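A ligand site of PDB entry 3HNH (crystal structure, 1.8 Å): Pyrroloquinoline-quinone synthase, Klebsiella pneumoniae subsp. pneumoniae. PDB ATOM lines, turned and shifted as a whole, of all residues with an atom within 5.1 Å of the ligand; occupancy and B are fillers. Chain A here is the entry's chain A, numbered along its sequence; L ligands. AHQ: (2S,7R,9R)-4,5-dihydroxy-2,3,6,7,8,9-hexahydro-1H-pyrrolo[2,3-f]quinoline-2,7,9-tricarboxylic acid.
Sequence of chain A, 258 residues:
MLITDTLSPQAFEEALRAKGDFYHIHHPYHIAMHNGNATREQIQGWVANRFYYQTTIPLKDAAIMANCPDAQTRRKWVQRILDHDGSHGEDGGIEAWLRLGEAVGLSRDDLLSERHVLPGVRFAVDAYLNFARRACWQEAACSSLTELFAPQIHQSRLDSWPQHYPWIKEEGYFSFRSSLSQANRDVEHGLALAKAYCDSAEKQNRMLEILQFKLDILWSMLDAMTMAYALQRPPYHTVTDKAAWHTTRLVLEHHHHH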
ATOM      1  N   TYR A  23      10.449   2.515 -10.131  1.00  0.00           N
ATOM      2  CA  TYR A  23       9.370   1.890 -10.841  1.00  0.00           C
ATOM      3  C   TYR A  23       8.884   0.682 -10.092  1.00  0.00           C
ATOM      4  O   TYR A  23       9.601   0.125  -9.286  1.00  0.00           O
ATOM      5  CB  TYR A  23       9.789   1.506 -12.237  1.00  0.00           C
ATOM      6  CG  TYR A  23       8.694   1.305 -13.240  1.00  0.00           C
ATOM      7  CD1 TYR A  23       7.701   2.241 -13.423  1.00  0.00           C
ATOM      8  CD2 TYR A  23       8.664   0.191 -14.013  1.00  0.00           C
ATOM      9  CE1 TYR A  23       6.739   2.065 -14.348  1.00  0.00           C
ATOM     10  CE2 TYR A  23       7.703   0.010 -14.947  1.00  0.00           C
ATOM     11  CZ  TYR A  23       6.746   0.944 -15.123  1.00  0.00           C
ATOM     12  OH  TYR A  23       5.777   0.754 -16.064  1.00  0.00           O
ATOM     13  N   HIS A  24       7.642   0.301 -10.351  1.00  0.00           N
ATOM     14  CA  HIS A  24       6.974  -0.681  -9.531  1.00  0.00           C
ATOM     15  C   HIS A  24       7.498  -2.119  -9.667  1.00  0.00           C
ATOM     16  O   HIS A  24       7.201  -2.939  -8.835  1.00  0.00           O
ATOM     17  CB  HIS A  24       5.443  -0.600  -9.621  1.00  0.00           C
ATOM     18  CG  HIS A  24       4.869  -0.875 -10.963  1.00  0.00           C
ATOM     19  ND1 HIS A  24       5.592  -0.788 -12.121  1.00  0.00           N
ATOM     20  CD2 HIS A  24       3.622  -1.207 -11.323  1.00  0.00           C
ATOM     21  CE1 HIS A  24       4.821  -1.081 -13.144  1.00  0.00           C
ATOM     22  NE2 HIS A  24       3.622  -1.330 -12.686  1.00  0.00           N
ATOM     23  N   ARG A  50      -5.503  -4.470 -11.133  1.00  0.00           N
ATOM     24  CA  ARG A  50      -4.894  -3.834 -12.262  1.00  0.00           C
ATOM     25  C   ARG A  50      -5.900  -3.488 -13.318  1.00  0.00           C
ATOM     26  O   ARG A  50      -5.767  -2.527 -14.001  1.00  0.00           O
ATOM     27  CB  ARG A  50      -3.811  -4.673 -12.875  1.00  0.00           C
ATOM     28  CG  ARG A  50      -2.433  -4.270 -12.524  1.00  0.00           C
ATOM     29  CD  ARG A  50      -2.130  -2.826 -12.916  1.00  0.00           C
ATOM     30  NE  ARG A  50      -1.950  -2.649 -14.334  1.00  0.00           N
ATOM     31  CZ  ARG A  50      -0.787  -2.717 -14.902  1.00  0.00           C
ATOM     32  NH1 ARG A  50       0.271  -2.964 -14.179  1.00  0.00           N
ATOM     33  NH2 ARG A  50      -0.670  -2.534 -16.182  1.00  0.00           N
ATOM     34  N   TYR A  53      -7.134   0.081 -13.082  1.00  0.00           N
ATOM     35  CA  TYR A  53      -6.210   0.999 -13.668  1.00  0.00           C
ATOM     36  C   TYR A  53      -6.465   1.038 -15.146  1.00  0.00           C
ATOM     37  O   TYR A  53      -6.619   2.070 -15.695  1.00  0.00           O
ATOM     38  CB  TYR A  53      -4.773   0.582 -13.357  1.00  0.00           C
ATOM     39  CG  TYR A  53      -3.690   1.492 -13.877  1.00  0.00           C
ATOM     40  CD1 TYR A  53      -3.368   2.665 -13.231  1.00  0.00           C
ATOM     41  CD2 TYR A  53      -2.970   1.172 -14.991  1.00  0.00           C
ATOM     42  CE1 TYR A  53      -2.385   3.479 -13.686  1.00  0.00           C
ATOM     43  CE2 TYR A  53      -1.978   1.991 -15.447  1.00  0.00           C
ATOM     44  CZ  TYR A  53      -1.698   3.139 -14.782  1.00  0.00           C
ATOM     45  OH  TYR A  53      -0.727   3.931 -15.238  1.00  0.00           O
ATOM     46  N   GLN A  54      -6.528  -0.107 -15.777  1.00  0.00           N
ATOM     47  CA  GLN A  54      -6.699  -0.131 -17.204  1.00  0.00           C
ATOM     48  C   GLN A  54      -8.000   0.462 -17.691  1.00  0.00           C
ATOM     49  O   GLN A  54      -8.047   1.015 -18.725  1.00  0.00           O
ATOM     50  CB  GLN A  54      -6.507  -1.523 -17.786  1.00  0.00           C
ATOM     51  CG  GLN A  54      -5.348  -2.245 -17.245  1.00  0.00           C
ATOM     52  CD  GLN A  54      -4.040  -1.740 -17.779  1.00  0.00           C
ATOM     53  OE1 GLN A  54      -3.956  -1.331 -18.881  1.00  0.00           O
ATOM     54  NE2 GLN A  54      -3.027  -1.807 -16.971  1.00  0.00           N
ATOM     55  N   ILE A  57      -7.515   4.424 -17.548  1.00  0.00           N
ATOM     56  CA  ILE A  57      -6.652   5.070 -18.511  1.00  0.00           C
ATOM     57  C   ILE A  57      -7.367   5.835 -19.605  1.00  0.00           C
ATOM     58  O   ILE A  57      -7.028   6.930 -19.864  1.00  0.00           O
ATOM     59  CB  ILE A  57      -5.687   4.085 -19.115  1.00  0.00           C
ATOM     60  CG1 ILE A  57      -4.788   3.528 -18.056  1.00  0.00           C
ATOM     61  CG2 ILE A  57      -4.823   4.750 -20.090  1.00  0.00           C
ATOM     62  CD1 ILE A  57      -3.883   2.541 -18.611  1.00  0.00           C
ATOM     63  N   LYS A  60      -8.763   8.893 -18.230  1.00  0.00           N
ATOM     64  CA  LYS A  60      -7.634   9.791 -17.970  1.00  0.00           C
ATOM     65  C   LYS A  60      -7.162  10.481 -19.236  1.00  0.00           C
ATOM     66  O   LYS A  60      -6.950  11.649 -19.241  1.00  0.00           O
ATOM     67  CB  LYS A  60      -6.517   9.003 -17.313  1.00  0.00           C
ATOM     68  CG  LYS A  60      -5.310   9.781 -16.921  1.00  0.00           C
ATOM     69  CD  LYS A  60      -4.317   9.879 -18.041  1.00  0.00           C
ATOM     70  CE  LYS A  60      -3.596   8.615 -18.330  1.00  0.00           C
ATOM     71  NZ  LYS A  60      -2.817   8.737 -19.523  1.00  0.00           N
ATOM     72  N   ASP A  61      -7.051   9.745 -20.307  1.00  0.00           N
ATOM     73  CA  ASP A  61      -6.650  10.307 -21.578  1.00  0.00           C
ATOM     74  C   ASP A  61      -7.663  11.259 -22.187  1.00  0.00           C
ATOM     75  O   ASP A  61      -7.336  12.208 -22.819  1.00  0.00           O
ATOM     76  CB  ASP A  61      -6.303   9.216 -22.563  1.00  0.00           C
ATOM     77  CG  ASP A  61      -4.972   8.562 -22.246  1.00  0.00           C
ATOM     78  OD1 ASP A  61      -4.087   9.267 -21.839  1.00  0.00           O
ATOM     79  OD2 ASP A  61      -4.836   7.371 -22.416  1.00  0.00           O
ATOM     80  N   ARG A  80      -4.410   6.825 -28.000  1.00  0.00           N
ATOM     81  CA  ARG A  80      -4.358   6.115 -26.765  1.00  0.00           C
ATOM     82  C   ARG A  80      -5.717   5.553 -26.405  1.00  0.00           C
ATOM     83  O   ARG A  80      -5.811   4.492 -25.879  1.00  0.00           O
ATOM     84  CB  ARG A  80      -3.843   7.005 -25.659  1.00  0.00           C
ATOM     85  CG  ARG A  80      -2.527   7.599 -25.975  1.00  0.00           C
ATOM     86  CD  ARG A  80      -2.100   8.621 -25.033  1.00  0.00           C
ATOM     87  NE  ARG A  80      -0.723   8.941 -25.327  1.00  0.00           N
ATOM     88  CZ  ARG A  80       0.297   8.460 -24.671  1.00  0.00           C
ATOM     89  NH1 ARG A  80       0.111   7.668 -23.662  1.00  0.00           N
ATOM     90  NH2 ARG A  80       1.512   8.791 -25.045  1.00  0.00           N
ATOM     91  N   HIS A  84      -7.047   1.522 -26.058  1.00  0.00           N
ATOM     92  CA  HIS A  84      -7.630   0.912 -24.894  1.00  0.00           C
ATOM     93  C   HIS A  84      -9.015   0.414 -25.142  1.00  0.00           C
ATOM     94  O   HIS A  84      -9.367  -0.661 -24.744  1.00  0.00           O
ATOM     95  CB  HIS A  84      -7.615   1.849 -23.722  1.00  0.00           C
ATOM     96  CG  HIS A  84      -6.241   2.160 -23.246  1.00  0.00           C
ATOM     97  ND1 HIS A  84      -5.390   1.202 -22.779  1.00  0.00           N
ATOM     98  CD2 HIS A  84      -5.548   3.322 -23.227  1.00  0.00           C
ATOM     99  CE1 HIS A  84      -4.232   1.741 -22.475  1.00  0.00           C
ATOM    100  NE2 HIS A  84      -4.306   3.028 -22.728  1.00  0.00           N
ATOM    101  N   TYR A 128      -4.876   9.574 -10.214  1.00  0.00           N
ATOM    102  CA  TYR A 128      -4.355   9.794 -11.532  1.00  0.00           C
ATOM    103  C   TYR A 128      -5.360  10.520 -12.415  1.00  0.00           C
ATOM    104  O   TYR A 128      -5.037  11.476 -13.053  1.00  0.00           O
ATOM    105  CB  TYR A 128      -3.961   8.483 -12.153  1.00  0.00           C
ATOM    106  CG  TYR A 128      -3.080   8.555 -13.369  1.00  0.00           C
ATOM    107  CD1 TYR A 128      -2.328   9.668 -13.665  1.00  0.00           C
ATOM    108  CD2 TYR A 128      -2.992   7.499 -14.218  1.00  0.00           C
ATOM    109  CE1 TYR A 128      -1.548   9.703 -14.770  1.00  0.00           C
ATOM    110  CE2 TYR A 128      -2.223   7.515 -15.301  1.00  0.00           C
ATOM    111  CZ  TYR A 128      -1.476   8.622 -15.582  1.00  0.00           C
ATOM    112  OH  TYR A 128      -0.705   8.628 -16.683  1.00  0.00           O
ATOM    113  N   SER A 143       3.055  12.923 -17.588  1.00  0.00           N
ATOM    114  CA  SER A 143       3.053  11.902 -16.576  1.00  0.00           C
ATOM    115  C   SER A 143       2.890  10.506 -17.133  1.00  0.00           C
ATOM    116  O   SER A 143       3.093   9.572 -16.445  1.00  0.00           O
ATOM    117  CB  SER A 143       2.017  12.166 -15.505  1.00  0.00           C
ATOM    118  OG  SER A 143       0.731  11.969 -15.987  1.00  0.00           O
ATOM    119  N   SER A 144       2.545  10.402 -18.387  1.00  0.00           N
ATOM    120  CA  SER A 144       2.408   9.113 -19.027  1.00  0.00           C
ATOM    121  C   SER A 144       3.750   8.463 -19.357  1.00  0.00           C
ATOM    122  O   SER A 144       3.803   7.347 -19.775  1.00  0.00           O
ATOM    123  CB  SER A 144       1.624   9.270 -20.310  1.00  0.00           C
ATOM    124  OG  SER A 144       2.358   9.918 -21.295  1.00  0.00           O
ATOM    125  N   THR A 146       6.116   7.249 -17.733  1.00  0.00           N
ATOM    126  CA  THR A 146       6.495   6.053 -17.048  1.00  0.00           C
ATOM    127  C   THR A 146       6.300   4.770 -17.842  1.00  0.00           C
ATOM    128  O   THR A 146       6.857   3.775 -17.507  1.00  0.00           O
ATOM    129  CB  THR A 146       5.833   5.919 -15.699  1.00  0.00           C
ATOM    130  OG1 THR A 146       4.445   5.718 -15.867  1.00  0.00           O
ATOM    131  CG2 THR A 146       6.087   7.117 -14.881  1.00  0.00           C
ATOM    132  N   GLU A 147       5.520   4.797 -18.906  1.00  0.00           N
ATOM    133  CA  GLU A 147       5.362   3.562 -19.664  1.00  0.00           C
ATOM    134  C   GLU A 147       6.670   3.203 -20.327  1.00  0.00           C
ATOM    135  O   GLU A 147       6.828   2.100 -20.759  1.00  0.00           O
ATOM    136  CB  GLU A 147       4.207   3.614 -20.662  1.00  0.00           C
ATOM    137  CG  GLU A 147       4.253   4.743 -21.614  1.00  0.00           C
ATOM    138  OE1 GLU A 147       2.107   4.097 -22.452  1.00  0.00           O
ATOM    139  OE2 GLU A 147       2.677   6.254 -22.555  1.00  0.00           O
ATOM    140  N   ALA A 150       8.922   0.390 -18.659  1.00  0.00           N
ATOM    141  CA  ALA A 150       8.584  -1.000 -18.823  1.00  0.00           C
ATOM    142  C   ALA A 150       9.500  -1.601 -19.866  1.00  0.00           C
ATOM    143  O   ALA A 150      10.697  -1.330 -19.843  1.00  0.00           O
ATOM    144  CB  ALA A 150       7.160  -1.143 -19.208  1.00  0.00           C
ATOM    145  N   ARG A 185      -0.206   3.918 -29.814  1.00  0.00           N
ATOM    146  CA  ARG A 185       0.160   5.170 -29.209  1.00  0.00           C
ATOM    147  C   ARG A 185       1.662   5.373 -29.272  1.00  0.00           C
ATOM    148  O   ARG A 185       2.412   4.417 -29.281  1.00  0.00           O
ATOM    149  CB  ARG A 185      -0.297   5.236 -27.770  1.00  0.00           C
ATOM    150  CG  ARG A 185       0.238   4.188 -26.889  1.00  0.00           C
ATOM    151  CD  ARG A 185      -0.428   4.230 -25.576  1.00  0.00           C
ATOM    152  NE  ARG A 185       0.036   3.225 -24.650  1.00  0.00           N
ATOM    153  CZ  ARG A 185      -0.455   1.999 -24.585  1.00  0.00           C
ATOM    154  NH1 ARG A 185      -1.399   1.635 -25.406  1.00  0.00           N
ATOM    155  NH2 ARG A 185       0.009   1.136 -23.708  1.00  0.00           N
ATOM    156  N   LYS A 214       3.287   9.852 -10.023  1.00  0.00           N
ATOM    157  CA  LYS A 214       2.839   8.737 -10.806  1.00  0.00           C
ATOM    158  C   LYS A 214       3.417   7.429 -10.316  1.00  0.00           C
ATOM    159  O   LYS A 214       2.747   6.449 -10.251  1.00  0.00           O
ATOM    160  CB  LYS A 214       3.134   8.945 -12.260  1.00  0.00           C
ATOM    161  CG  LYS A 214       2.895   7.777 -13.106  1.00  0.00           C
ATOM    162  CD  LYS A 214       1.515   7.690 -13.624  1.00  0.00           C
ATOM    163  CE  LYS A 214       1.420   6.672 -14.689  1.00  0.00           C
ATOM    164  NZ  LYS A 214       1.902   7.114 -15.969  1.00  0.00           N
ATOM    165  N   LEU A 218       1.477   3.838  -8.601  1.00  0.00           N
ATOM    166  CA  LEU A 218       1.743   2.444  -8.900  1.00  0.00           C
ATOM    167  C   LEU A 218       2.225   1.628  -7.719  1.00  0.00           C
ATOM    168  O   LEU A 218       1.830   0.531  -7.550  1.00  0.00           O
ATOM    169  CB  LEU A 218       2.701   2.334 -10.053  1.00  0.00           C
ATOM    170  CG  LEU A 218       2.346   2.997 -11.369  1.00  0.00           C
ATOM    171  CD1 LEU A 218       3.534   3.084 -12.261  1.00  0.00           C
ATOM    172  CD2 LEU A 218       1.196   2.401 -12.073  1.00  0.00           C
HETATM  173  O5  AHQ L   1      -0.347  -1.017 -19.793  1.00  0.00           O
HETATM  174  C5  AHQ L   1      -0.073   0.113 -19.400  1.00  0.00           C
HETATM  175  C4  AHQ L   1      -0.627   1.207 -20.006  1.00  0.00           C
HETATM  176  O4  AHQ L   1      -1.378   0.988 -20.941  1.00  0.00           O
HETATM  177  C3A AHQ L   1      -0.303   2.480 -19.550  1.00  0.00           C
HETATM  178  C3  AHQ L   1      -0.790   3.822 -20.069  1.00  0.00           C
HETATM  179  C2  AHQ L   1       0.215   4.739 -19.405  1.00  0.00           C
HETATM  180  C2X AHQ L   1      -0.465   6.057 -19.035  1.00  0.00           C
HETATM  181  O2B AHQ L   1      -0.185   6.593 -17.980  1.00  0.00           O
HETATM  182  O2A AHQ L   1      -1.227   6.499 -19.850  1.00  0.00           O
HETATM  183  N1  AHQ L   1       0.678   3.976 -18.247  1.00  0.00           N
HETATM  184  C1A AHQ L   1       0.572   2.669 -18.471  1.00  0.00           C
HETATM  185  C9A AHQ L   1       1.133   1.539 -17.866  1.00  0.00           C
HETATM  186  C6A AHQ L   1       0.778   0.279 -18.335  1.00  0.00           C
HETATM  187  N6  AHQ L   1       1.277  -0.879 -17.794  1.00  0.00           N
HETATM  188  C7  AHQ L   1       2.190  -0.886 -16.662  1.00  0.00           C
HETATM  189  C7X AHQ L   1       3.042  -2.168 -16.718  1.00  0.00           C
HETATM  190  O7B AHQ L   1       2.622  -3.076 -17.445  1.00  0.00           O
HETATM  191  O7A AHQ L   1       4.050  -2.224 -15.989  1.00  0.00           O
HETATM  192  C8  AHQ L   1       3.025   0.385 -16.685  1.00  0.00           C
HETATM  193  C9  AHQ L   1       2.074   1.569 -16.645  1.00  0.00           C
HETATM  194  C9X AHQ L   1       2.828   2.873 -16.396  1.00  0.00           C
HETATM  195  O9B AHQ L   1       4.041   2.845 -16.367  1.00  0.00           O
HETATM  196  O9A AHQ L   1       2.139   3.845 -16.126  1.00  0.00           O
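The side-chain hydroxyl of Tyr 128 is in hydrogen-bond range of an oxygen (O2B) of the ligand, 2.5 Å away.
The side-chain hydroxyl (OH) of Tyr 23 lies within hydrogen-bond range of an oxygen (O9B) of the ligand, 2.7 Å away.
The side-chain amino group of Lys 60 lies within salt-bridge range of an oxygen (O2A) of the ligand (2.8 Å).
OG1 of Thr 146 is in hydrogen-bond range of O9B of the ligand, 2.9 Å away.
O2B of the ligand is in salt-bridge range of NZ of Lys 214 (2.9 Å).
O9A of the ligand lies within hydrogen-bond range of OH of Tyr 53 (3.0 Å).
NH2 of Arg 50 lies within salt-bridge range of O7B of the ligand (3.6 Å).
An oxygen (O4) of the ligand is in hydrogen-bond range of the guanidinium group (NH2) of Arg 185 (3.1 Å).
NE2 of His 24 sits close to O7A of the ligand, at 3.4 Å.
OH of Tyr 128 sits at hydrogen-bond distance from NZ of Lys 214, 3.1 Å away.
NZ of Lys 60 lies within salt-bridge range of OD1 of Asp 61 (2.7 Å).
The side-chain hydroxyl (OG1) of Thr 146 is in hydrogen-bond range of the side-chain amino group (NZ) of Lys 214.
The side-chain amino group of Lys 214 is in hydrogen-bond range of the backbone carbonyl oxygen of Ser 143.
The guanidinium group of Arg 50 lies close to the side-chain amide nitrogen of Gln 54 (2.6 Å).
The guanidinium group of Arg 185 is in salt-bridge range of the side-chain carboxylate of Glu 147 (3.1 Å).
The side-chain carboxylate of Glu 147 lies within salt-bridge range of the guanidinium group of Arg 80.
Residues that only touch the ligand: His 84 (3.3 Å), Glu 147 (3.5 Å), Ile 57 (3.7 Å), Gln 54 (3.7 Å) and Ser 144 (3.8 Å).
Hydrophobic or aromatic side chains within 4 Å of the ligand: Tyr 23, His 24, Tyr 53, Ile 57, His 84 and Tyr 128.
Of the 19 residues printed, 14 come within 4 Å of the ligand.
The nearest printed residue that does not touch the ligand is Leu 218 (4.1 Å).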
